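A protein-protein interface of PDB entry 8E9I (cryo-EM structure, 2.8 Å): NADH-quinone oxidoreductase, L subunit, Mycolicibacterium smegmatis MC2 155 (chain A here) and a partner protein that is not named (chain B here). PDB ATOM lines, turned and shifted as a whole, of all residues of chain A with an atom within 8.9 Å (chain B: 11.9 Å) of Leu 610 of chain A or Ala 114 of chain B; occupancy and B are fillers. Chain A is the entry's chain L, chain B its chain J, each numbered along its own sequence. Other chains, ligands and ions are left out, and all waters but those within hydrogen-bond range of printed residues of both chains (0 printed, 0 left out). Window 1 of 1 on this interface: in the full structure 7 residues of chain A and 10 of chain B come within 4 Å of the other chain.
Leu 610 of chain A touches just these residues of chain B: His 107, Ala 110, Ala 111 and Ala 114. Of the printed residues of chain A, Ala 114 of chain B touches Leu 610 (3.9 Å). No residue of chain B comes within 4 Å of Ser 607 of chain A. No residue of chain B comes within 4 Å of Ala 609 of chain A. No residue of chain B comes within 4 Å of Ser 611 of chain A. No residue of chain B comes within 4 Å of Met 612 of chain A. No residue of chain B comes within 4 Å of Gly 614 of chain A. Of chain B, only Phe 118 (3.5 Å) and Leu 121 (3.9 Å) come within 4 Å of Ser 616 of chain A. Ala 111 of chain B touches just one residue of chain A: Leu 610 (3.8 Å). Gly 115 of chain B touches just one residue of chain A: Leu 613 (3.7 Å). Printed residues of chain A within 4 Å of Thr 103 of chain B: Arg 606 (3.8 Å). Of the printed residues of chain B, Leu 613 of chain A touches Gly 115 (3.7 Å) and Phe 118 (3.98 Å). Ile 120 of chain B touches none of the printed residues of chain A. Gly 119 of chain B touches none of the printed residues of chain A. The nearest residue of chain A that does not touch Ala 114 of chain B is Leu 613 of chain A (4.1 Å).
The backbone NH (N) of Phe 604 of chain A lies close to the side-chain hydroxyl (OG1) of Thr 602 of chain A, at 3.4 Å. O of Phe 604 of chain A sits at hydrogen-bond distance from OG of Ser 607 of chain A. The backbone carbonyl oxygen (O) of Leu 613 of chain A sits at hydrogen-bond distance from the side-chain hydroxyl (OG) of Ser 616 of chain A, 3.1 Å away.
Among the printed residues, pairs that only touch across the chains: Arg 606 of chain A with His 107 of chain B (3.5 Å), Ser 616 of chain A with Phe 118 of chain B (3.5 Å), Phe 604 of chain A with Ile 104 of chain B (3.5 Å), Leu 610 of chain A with His 107 of chain B (3.6 Å), Arg 606 of chain A with Ile 104 of chain B (3.6 Å), Leu 610 of chain A with Ala 110 of chain B (3.7 Å), Leu 613 of chain A with Gly 115 of chain B (3.7 Å), Leu 610 of chain A with Ala 111 of chain B (3.8 Å), Arg 606 of chain A with Thr 103 of chain B (3.8 Å), Ser 616 of chain A with Leu 121 of chain B (3.9 Å), Leu 610 of chain A with Ala 114 of chain B (3.9 Å) and Leu 613 of chain A with Phe 118 of chain B (3.98 Å).
Printed residues of chain B that touch a printed residue of chain A: Thr 103, Ile 104, His 107, Ala 110, Ala 111, Ala 114, Gly 115, Phe 118 and Leu 121. Hydrophobic or aromatic side chains of chain B within 4 Å of the printed part of chain A: Ile 104, His 107, Ala 110, Ala 114, Phe 118 and Leu 121. Of the 15 printed residues of chain A, 5 touch a printed residue of chain B. Hydrophobic or aromatic side chains of chain A within 4 Å of the printed part of chain B: Phe 604, Leu 610 and Leu 613. Among the printed residues, no Asp or Glu carboxylate lies within 4 Å of a Lys or Arg side-chain nitrogen of the other chain.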
ATOM      1  N   THR A 602      14.616  25.453 -10.615  1.00  0.00           N
ATOM      2  CA  THR A 602      15.241  26.635 -10.042  1.00  0.00           C
ATOM      3  C   THR A 602      16.455  27.083 -10.839  1.00  0.00           C
ATOM      4  O   THR A 602      16.945  28.196 -10.627  1.00  0.00           O
ATOM      5  CB  THR A 602      15.645  26.359  -8.597  1.00  0.00           C
ATOM      6  OG1 THR A 602      16.742  25.437  -8.573  1.00  0.00           O
ATOM      7  CG2 THR A 602      14.477  25.771  -7.824  1.00  0.00           C
ATOM      8  N   PHE A 604      19.409  25.879 -10.583  1.00  0.00           N
ATOM      9  CA  PHE A 604      20.627  25.517  -9.876  1.00  0.00           C
ATOM     10  C   PHE A 604      20.940  24.049 -10.121  1.00  0.00           C
ATOM     11  O   PHE A 604      20.173  23.169  -9.719  1.00  0.00           O
ATOM     12  CB  PHE A 604      20.478  25.792  -8.386  1.00  0.00           C
ATOM     13  CG  PHE A 604      20.424  27.247  -8.046  1.00  0.00           C
ATOM     14  CD1 PHE A 604      21.561  28.029  -8.130  1.00  0.00           C
ATOM     15  CD2 PHE A 604      19.243  27.835  -7.649  1.00  0.00           C
ATOM     16  CE1 PHE A 604      21.517  29.370  -7.816  1.00  0.00           C
ATOM     17  CE2 PHE A 604      19.194  29.174  -7.334  1.00  0.00           C
ATOM     18  CZ  PHE A 604      20.331  29.943  -7.419  1.00  0.00           C
ATOM     19  N   ALA A 605      22.082  23.788 -10.757  1.00  0.00           N
ATOM     20  CA  ALA A 605      22.450  22.414 -11.072  1.00  0.00           C
ATOM     21  C   ALA A 605      22.456  21.547  -9.827  1.00  0.00           C
ATOM     22  O   ALA A 605      22.195  20.342  -9.907  1.00  0.00           O
ATOM     23  CB  ALA A 605      23.823  22.380 -11.738  1.00  0.00           C
ATOM     24  N   ARG A 606      22.750  22.135  -8.672  1.00  0.00           N
ATOM     25  CA  ARG A 606      22.748  21.362  -7.441  1.00  0.00           C
ATOM     26  C   ARG A 606      21.334  21.004  -7.015  1.00  0.00           C
ATOM     27  O   ARG A 606      21.123  19.962  -6.394  1.00  0.00           O
ATOM     28  CB  ARG A 606      23.474  22.138  -6.349  1.00  0.00           C
ATOM     29  CG  ARG A 606      24.933  22.380  -6.680  1.00  0.00           C
ATOM     30  CD  ARG A 606      25.686  22.949  -5.512  1.00  0.00           C
ATOM     31  NE  ARG A 606      25.003  24.110  -4.955  1.00  0.00           N
ATOM     32  CZ  ARG A 606      24.697  24.268  -3.675  1.00  0.00           C
ATOM     33  NH1 ARG A 606      25.045  23.378  -2.760  1.00  0.00           N
ATOM     34  NH2 ARG A 606      24.027  25.353  -3.302  1.00  0.00           N
ATOM     35  N   SER A 607      20.344  21.829  -7.358  1.00  0.00           N
ATOM     36  CA  SER A 607      18.963  21.440  -7.097  1.00  0.00           C
ATOM     37  C   SER A 607      18.535  20.283  -7.990  1.00  0.00           C
ATOM     38  O   SER A 607      17.859  19.354  -7.527  1.00  0.00           O
ATOM     39  CB  SER A 607      18.035  22.634  -7.294  1.00  0.00           C
ATOM     40  OG  SER A 607      17.874  22.923  -8.669  1.00  0.00           O
ATOM     41  N   TYR A 608      18.917  20.318  -9.265  1.00  0.00           N
ATOM     42  CA  TYR A 608      18.644  19.184 -10.136  1.00  0.00           C
ATOM     43  C   TYR A 608      19.324  17.931  -9.610  1.00  0.00           C
ATOM     44  O   TYR A 608      18.740  16.840  -9.620  1.00  0.00           O
ATOM     45  CB  TYR A 608      19.127  19.480 -11.550  1.00  0.00           C
ATOM     46  CG  TYR A 608      18.550  20.722 -12.182  1.00  0.00           C
ATOM     47  CD1 TYR A 608      17.444  21.360 -11.644  1.00  0.00           C
ATOM     48  CD2 TYR A 608      19.119  21.256 -13.324  1.00  0.00           C
ATOM     49  CE1 TYR A 608      16.926  22.487 -12.229  1.00  0.00           C
ATOM     50  CE2 TYR A 608      18.612  22.376 -13.912  1.00  0.00           C
ATOM     51  CZ  TYR A 608      17.517  22.991 -13.363  1.00  0.00           C
ATOM     52  OH  TYR A 608      17.018  24.114 -13.968  1.00  0.00           O
ATOM     53  N   ALA A 609      20.567  18.073  -9.153  1.00  0.00           N
ATOM     54  CA  ALA A 609      21.271  16.943  -8.568  1.00  0.00           C
ATOM     55  C   ALA A 609      20.571  16.460  -7.309  1.00  0.00           C
ATOM     56  O   ALA A 609      20.576  15.264  -7.012  1.00  0.00           O
ATOM     57  CB  ALA A 609      22.715  17.332  -8.266  1.00  0.00           C
ATOM     58  N   LEU A 610      19.989  17.377  -6.539  1.00  0.00           N
ATOM     59  CA  LEU A 610      19.247  16.977  -5.352  1.00  0.00           C
ATOM     60  C   LEU A 610      18.032  16.148  -5.729  1.00  0.00           C
ATOM     61  O   LEU A 610      17.723  15.150  -5.071  1.00  0.00           O
ATOM     62  CB  LEU A 610      18.832  18.210  -4.551  1.00  0.00           C
ATOM     63  CG  LEU A 610      17.812  17.996  -3.434  1.00  0.00           C
ATOM     64  CD1 LEU A 610      18.337  17.030  -2.391  1.00  0.00           C
ATOM     65  CD2 LEU A 610      17.464  19.326  -2.797  1.00  0.00           C
ATOM     66  N   SER A 611      17.325  16.551  -6.783  1.00  0.00           N
ATOM     67  CA  SER A 611      16.212  15.735  -7.259  1.00  0.00           C
ATOM     68  C   SER A 611      16.699  14.361  -7.697  1.00  0.00           C
ATOM     69  O   SER A 611      16.096  13.337  -7.359  1.00  0.00           O
ATOM     70  CB  SER A 611      15.494  16.434  -8.410  1.00  0.00           C
ATOM     71  OG  SER A 611      14.948  17.670  -7.996  1.00  0.00           O
ATOM     72  N   MET A 612      17.807  14.319  -8.430  1.00  0.00           N
ATOM     73  CA  MET A 612      18.338  13.042  -8.888  1.00  0.00           C
ATOM     74  C   MET A 612      18.731  12.146  -7.719  1.00  0.00           C
ATOM     75  O   MET A 612      18.460  10.942  -7.746  1.00  0.00           O
ATOM     76  CB  MET A 612      19.531  13.289  -9.807  1.00  0.00           C
ATOM     77  CG  MET A 612      19.114  13.814 -11.172  1.00  0.00           C
ATOM     78  SD  MET A 612      20.205  13.342 -12.510  1.00  0.00           S
ATOM     79  CE  MET A 612      21.767  13.840 -11.837  1.00  0.00           C
ATOM     80  N   LEU A 613      19.367  12.709  -6.689  1.00  0.00           N
ATOM     81  CA  LEU A 613      19.738  11.933  -5.512  1.00  0.00           C
ATOM     82  C   LEU A 613      18.520  11.481  -4.720  1.00  0.00           C
ATOM     83  O   LEU A 613      18.513  10.367  -4.190  1.00  0.00           O
ATOM     84  CB  LEU A 613      20.668  12.743  -4.611  1.00  0.00           C
ATOM     85  CG  LEU A 613      21.200  12.010  -3.378  1.00  0.00           C
ATOM     86  CD1 LEU A 613      21.943  10.743  -3.759  1.00  0.00           C
ATOM     87  CD2 LEU A 613      22.099  12.921  -2.569  1.00  0.00           C
ATOM     88  N   GLY A 614      17.495  12.325  -4.613  1.00  0.00           N
ATOM     89  CA  GLY A 614      16.224  11.865  -4.090  1.00  0.00           C
ATOM     90  C   GLY A 614      15.620  10.779  -4.944  1.00  0.00           C
ATOM     91  O   GLY A 614      14.757  10.031  -4.475  1.00  0.00           O
ATOM     92  N   GLY A 615      16.063  10.673  -6.194  1.00  0.00           N
ATOM     93  CA  GLY A 615      15.752   9.518  -7.016  1.00  0.00           C
ATOM     94  C   GLY A 615      16.022   8.190  -6.338  1.00  0.00           C
ATOM     95  O   GLY A 615      15.578   7.156  -6.846  1.00  0.00           O
ATOM     96  N   SER A 616      16.731   8.191  -5.203  1.00  0.00           N
ATOM     97  CA  SER A 616      16.778   7.014  -4.343  1.00  0.00           C
ATOM     98  C   SER A 616      15.386   6.563  -3.938  1.00  0.00           C
ATOM     99  O   SER A 616      15.237   5.506  -3.315  1.00  0.00           O
ATOM    100  CB  SER A 616      17.597   7.302  -3.090  1.00  0.00           C
ATOM    101  OG  SER A 616      17.006   8.345  -2.340  1.00  0.00           O
ATOM    102  N   ALA A 617      14.365   7.362  -4.247  1.00  0.00           N
ATOM    103  CA  ALA A 617      13.008   6.845  -4.249  1.00  0.00           C
ATOM    104  C   ALA A 617      12.935   5.569  -5.074  1.00  0.00           C
ATOM    105  O   ALA A 617      12.259   4.610  -4.692  1.00  0.00           O
ATOM    106  CB  ALA A 617      12.047   7.901  -4.796  1.00  0.00           C
ATOM    107  N   GLU B 102      24.611  27.909   3.033  1.00  0.00           N
ATOM    108  CA  GLU B 102      23.500  27.546   2.166  1.00  0.00           C
ATOM    109  C   GLU B 102      22.939  28.786   1.483  1.00  0.00           C
ATOM    110  O   GLU B 102      22.490  29.723   2.148  1.00  0.00           O
ATOM    111  CB  GLU B 102      22.414  26.848   2.979  1.00  0.00           C
ATOM    112  N   THR B 103      22.973  28.791   0.151  1.00  0.00           N
ATOM    113  CA  THR B 103      22.412  29.893  -0.618  1.00  0.00           C
ATOM    114  C   THR B 103      21.040  29.576  -1.187  1.00  0.00           C
ATOM    115  O   THR B 103      20.324  30.500  -1.588  1.00  0.00           O
ATOM    116  CB  THR B 103      23.346  30.273  -1.766  1.00  0.00           C
ATOM    117  OG1 THR B 103      23.814  29.088  -2.418  1.00  0.00           O
ATOM    118  CG2 THR B 103      24.533  31.052  -1.242  1.00  0.00           C
ATOM    119  N   ILE B 104      20.662  28.305  -1.236  1.00  0.00           N
ATOM    120  CA  ILE B 104      19.365  27.876  -1.745  1.00  0.00           C
ATOM    121  C   ILE B 104      18.511  27.497  -0.544  1.00  0.00           C
ATOM    122  O   ILE B 104      18.908  26.648   0.264  1.00  0.00           O
ATOM    123  CB  ILE B 104      19.502  26.707  -2.729  1.00  0.00           C
ATOM    124  CG1 ILE B 104      20.327  27.133  -3.944  1.00  0.00           C
ATOM    125  CG2 ILE B 104      18.130  26.214  -3.161  1.00  0.00           C
ATOM    126  CD1 ILE B 104      20.823  25.982  -4.784  1.00  0.00           C
ATOM    127  N   LYS B 105      17.342  28.118  -0.433  1.00  0.00           N
ATOM    128  CA  LYS B 105      16.561  28.050   0.795  1.00  0.00           C
ATOM    129  C   LYS B 105      16.329  26.608   1.217  1.00  0.00           C
ATOM    130  O   LYS B 105      15.648  25.848   0.525  1.00  0.00           O
ATOM    131  CB  LYS B 105      15.224  28.766   0.598  1.00  0.00           C
ATOM    132  N   GLY B 106      16.897  26.239   2.360  1.00  0.00           N
ATOM    133  CA  GLY B 106      16.716  24.912   2.902  1.00  0.00           C
ATOM    134  C   GLY B 106      17.381  23.812   2.116  1.00  0.00           C
ATOM    135  O   GLY B 106      17.144  22.637   2.411  1.00  0.00           O
ATOM    136  N   HIS B 107      18.203  24.148   1.124  1.00  0.00           N
ATOM    137  CA  HIS B 107      18.817  23.117   0.299  1.00  0.00           C
ATOM    138  C   HIS B 107      19.759  22.240   1.107  1.00  0.00           C
ATOM    139  O   HIS B 107      19.863  21.040   0.852  1.00  0.00           O
ATOM    140  CB  HIS B 107      19.564  23.753  -0.868  1.00  0.00           C
ATOM    141  CG  HIS B 107      20.374  22.778  -1.662  1.00  0.00           C
ATOM    142  ND1 HIS B 107      19.827  21.977  -2.638  1.00  0.00           N
ATOM    143  CD2 HIS B 107      21.693  22.476  -1.623  1.00  0.00           C
ATOM    144  CE1 HIS B 107      20.772  21.223  -3.167  1.00  0.00           C
ATOM    145  NE2 HIS B 107      21.914  21.506  -2.568  1.00  0.00           N
ATOM    146  N   ARG B 108      20.476  22.821   2.069  1.00  0.00           N
ATOM    147  CA  ARG B 108      21.458  22.041   2.814  1.00  0.00           C
ATOM    148  C   ARG B 108      20.788  20.894   3.555  1.00  0.00           C
ATOM    149  O   ARG B 108      21.267  19.756   3.530  1.00  0.00           O
ATOM    150  CB  ARG B 108      22.216  22.945   3.786  1.00  0.00           C
ATOM    151  N   ILE B 109      19.660  21.170   4.208  1.00  0.00           N
ATOM    152  CA  ILE B 109      18.967  20.126   4.957  1.00  0.00           C
ATOM    153  C   ILE B 109      18.422  19.069   4.008  1.00  0.00           C
ATOM    154  O   ILE B 109      18.489  17.867   4.287  1.00  0.00           O
ATOM    155  CB  ILE B 109      17.850  20.734   5.824  1.00  0.00           C
ATOM    156  CG1 ILE B 109      18.452  21.600   6.928  1.00  0.00           C
ATOM    157  CG2 ILE B 109      17.003  19.635   6.432  1.00  0.00           C
ATOM    158  CD1 ILE B 109      17.472  22.576   7.543  1.00  0.00           C
ATOM    159  N   ALA B 110      17.861  19.498   2.878  1.00  0.00           N
ATOM    160  CA  ALA B 110      17.330  18.535   1.919  1.00  0.00           C
ATOM    161  C   ALA B 110      18.434  17.641   1.374  1.00  0.00           C
ATOM    162  O   ALA B 110      18.248  16.430   1.231  1.00  0.00           O
ATOM    163  CB  ALA B 110      16.619  19.263   0.782  1.00  0.00           C
ATOM    164  N   ALA B 111      19.591  18.220   1.060  1.00  0.00           N
ATOM    165  CA  ALA B 111      20.705  17.424   0.562  1.00  0.00           C
ATOM    166  C   ALA B 111      21.207  16.458   1.623  1.00  0.00           C
ATOM    167  O   ALA B 111      21.489  15.294   1.326  1.00  0.00           O
ATOM    168  CB  ALA B 111      21.835  18.339   0.093  1.00  0.00           C
ATOM    169  N   LEU B 112      21.329  16.919   2.868  1.00  0.00           N
ATOM    170  CA  LEU B 112      21.761  16.021   3.931  1.00  0.00           C
ATOM    171  C   LEU B 112      20.782  14.870   4.095  1.00  0.00           C
ATOM    172  O   LEU B 112      21.188  13.708   4.214  1.00  0.00           O
ATOM    173  CB  LEU B 112      21.907  16.790   5.242  1.00  0.00           C
ATOM    174  N   ILE B 113      19.484  15.169   4.077  1.00  0.00           N
ATOM    175  CA  ILE B 113      18.475  14.128   4.233  1.00  0.00           C
ATOM    176  C   ILE B 113      18.544  13.144   3.077  1.00  0.00           C
ATOM    177  O   ILE B 113      18.511  11.927   3.279  1.00  0.00           O
ATOM    178  CB  ILE B 113      17.075  14.753   4.347  1.00  0.00           C
ATOM    179  CG1 ILE B 113      16.928  15.472   5.687  1.00  0.00           C
ATOM    180  CG2 ILE B 113      16.010  13.682   4.187  1.00  0.00           C
ATOM    181  CD1 ILE B 113      15.777  16.447   5.721  1.00  0.00           C
ATOM    182  N   ALA B 114      18.625  13.653   1.848  1.00  0.00           N
ATOM    183  CA  ALA B 114      18.638  12.772   0.686  1.00  0.00           C
ATOM    184  C   ALA B 114      19.882  11.897   0.669  1.00  0.00           C
ATOM    185  O   ALA B 114      19.800  10.698   0.384  1.00  0.00           O
ATOM    186  CB  ALA B 114      18.546  13.592  -0.598  1.00  0.00           C
ATOM    187  N   GLY B 115      21.041  12.471   0.972  1.00  0.00           N
ATOM    188  CA  GLY B 115      22.262  11.698   1.014  1.00  0.00           C
ATOM    189  C   GLY B 115      22.213  10.633   2.084  1.00  0.00           C
ATOM    190  O   GLY B 115      22.570   9.480   1.832  1.00  0.00           O
ATOM    191  N   ALA B 116      21.770  11.001   3.288  1.00  0.00           N
ATOM    192  CA  ALA B 116      21.682  10.025   4.365  1.00  0.00           C
ATOM    193  C   ALA B 116      20.690   8.926   4.018  1.00  0.00           C
ATOM    194  O   ALA B 116      20.946   7.744   4.265  1.00  0.00           O
ATOM    195  CB  ALA B 116      21.286  10.717   5.668  1.00  0.00           C
ATOM    196  N   GLY B 117      19.546   9.296   3.448  1.00  0.00           N
ATOM    197  CA  GLY B 117      18.563   8.294   3.083  1.00  0.00           C
ATOM    198  C   GLY B 117      19.084   7.343   2.026  1.00  0.00           C
ATOM    199  O   GLY B 117      18.892   6.130   2.114  1.00  0.00           O
ATOM    200  N   PHE B 118      19.750   7.882   1.010  1.00  0.00           N
ATOM    201  CA  PHE B 118      20.311   7.028  -0.027  1.00  0.00           C
ATOM    202  C   PHE B 118      21.370   6.102   0.550  1.00  0.00           C
ATOM    203  O   PHE B 118      21.434   4.921   0.200  1.00  0.00           O
ATOM    204  CB  PHE B 118      20.886   7.883  -1.155  1.00  0.00           C
ATOM    205  CG  PHE B 118      21.648   7.101  -2.173  1.00  0.00           C
ATOM    206  CD1 PHE B 118      20.986   6.389  -3.152  1.00  0.00           C
ATOM    207  CD2 PHE B 118      23.028   7.087  -2.159  1.00  0.00           C
ATOM    208  CE1 PHE B 118      21.686   5.666  -4.092  1.00  0.00           C
ATOM    209  CE2 PHE B 118      23.733   6.367  -3.095  1.00  0.00           C
ATOM    210  CZ  PHE B 118      23.062   5.656  -4.064  1.00  0.00           C
ATOM    211  N   GLY B 119      22.211   6.618   1.445  1.00  0.00           N
ATOM    212  CA  GLY B 119      23.209   5.767   2.070  1.00  0.00           C
ATOM    213  C   GLY B 119      22.583   4.660   2.893  1.00  0.00           C
ATOM    214  O   GLY B 119      22.989   3.499   2.811  1.00  0.00           O
ATOM    215  N   ILE B 120      21.576   5.005   3.693  1.00  0.00           N
ATOM    216  CA  ILE B 120      20.896   4.004   4.507  1.00  0.00           C
ATOM    217  C   ILE B 120      20.259   2.951   3.614  1.00  0.00           C
ATOM    218  O   ILE B 120      20.336   1.749   3.888  1.00  0.00           O
ATOM    219  CB  ILE B 120      19.850   4.673   5.417  1.00  0.00           C
ATOM    220  CG1 ILE B 120      20.522   5.581   6.450  1.00  0.00           C
ATOM    221  CG2 ILE B 120      18.996   3.622   6.106  1.00  0.00           C
ATOM    222  CD1 ILE B 120      21.367   4.863   7.470  1.00  0.00           C
ATOM    223  N   LEU B 121      19.616   3.387   2.531  1.00  0.00           N
ATOM    224  CA  LEU B 121      18.938   2.451   1.644  1.00  0.00           C
ATOM    225  C   LEU B 121      19.930   1.547   0.928  1.00  0.00           C
ATOM    226  O   LEU B 121      19.666   0.355   0.743  1.00  0.00           O
ATOM    227  CB  LEU B 121      18.092   3.223   0.637  1.00  0.00           C
ATOM    228  CG  LEU B 121      16.908   3.956   1.259  1.00  0.00           C
ATOM    229  CD1 LEU B 121      16.421   5.050   0.337  1.00  0.00           C
ATOM    230  CD2 LEU B 121      15.784   2.989   1.576  1.00  0.00           C
ATOM    231  N   VAL B 122      21.073   2.091   0.510  1.00  0.00           N
ATOM    232  CA  VAL B 122      22.077   1.278  -0.168  1.00  0.00           C
ATOM    233  C   VAL B 122      22.674   0.271   0.801  1.00  0.00           C
ATOM    234  O   VAL B 122      22.947  -0.879   0.439  1.00  0.00           O
ATOM    235  CB  VAL B 122      23.162   2.172  -0.792  1.00  0.00           C
ATOM    236  CG1 VAL B 122      24.389   1.355  -1.127  1.00  0.00           C
ATOM    237  CG2 VAL B 122      22.633   2.853  -2.034  1.00  0.00           C
ATOM    238  N   ILE B 123      22.896   0.686   2.046  1.00  0.00           N
ATOM    239  CA  ILE B 123      23.385  -0.255   3.047  1.00  0.00           C
ATOM    240  C   ILE B 123      22.361  -1.353   3.274  1.00  0.00           C
ATOM    241  O   ILE B 123      22.707  -2.537   3.370  1.00  0.00           O
ATOM    242  CB  ILE B 123      23.731   0.483   4.351  1.00  0.00           C
ATOM    243  CG1 ILE B 123      25.002   1.311   4.157  1.00  0.00           C
ATOM    244  CG2 ILE B 123      23.911  -0.507   5.484  1.00  0.00           C
ATOM    245  CD1 ILE B 123      25.205   2.372   5.205  1.00  0.00           C
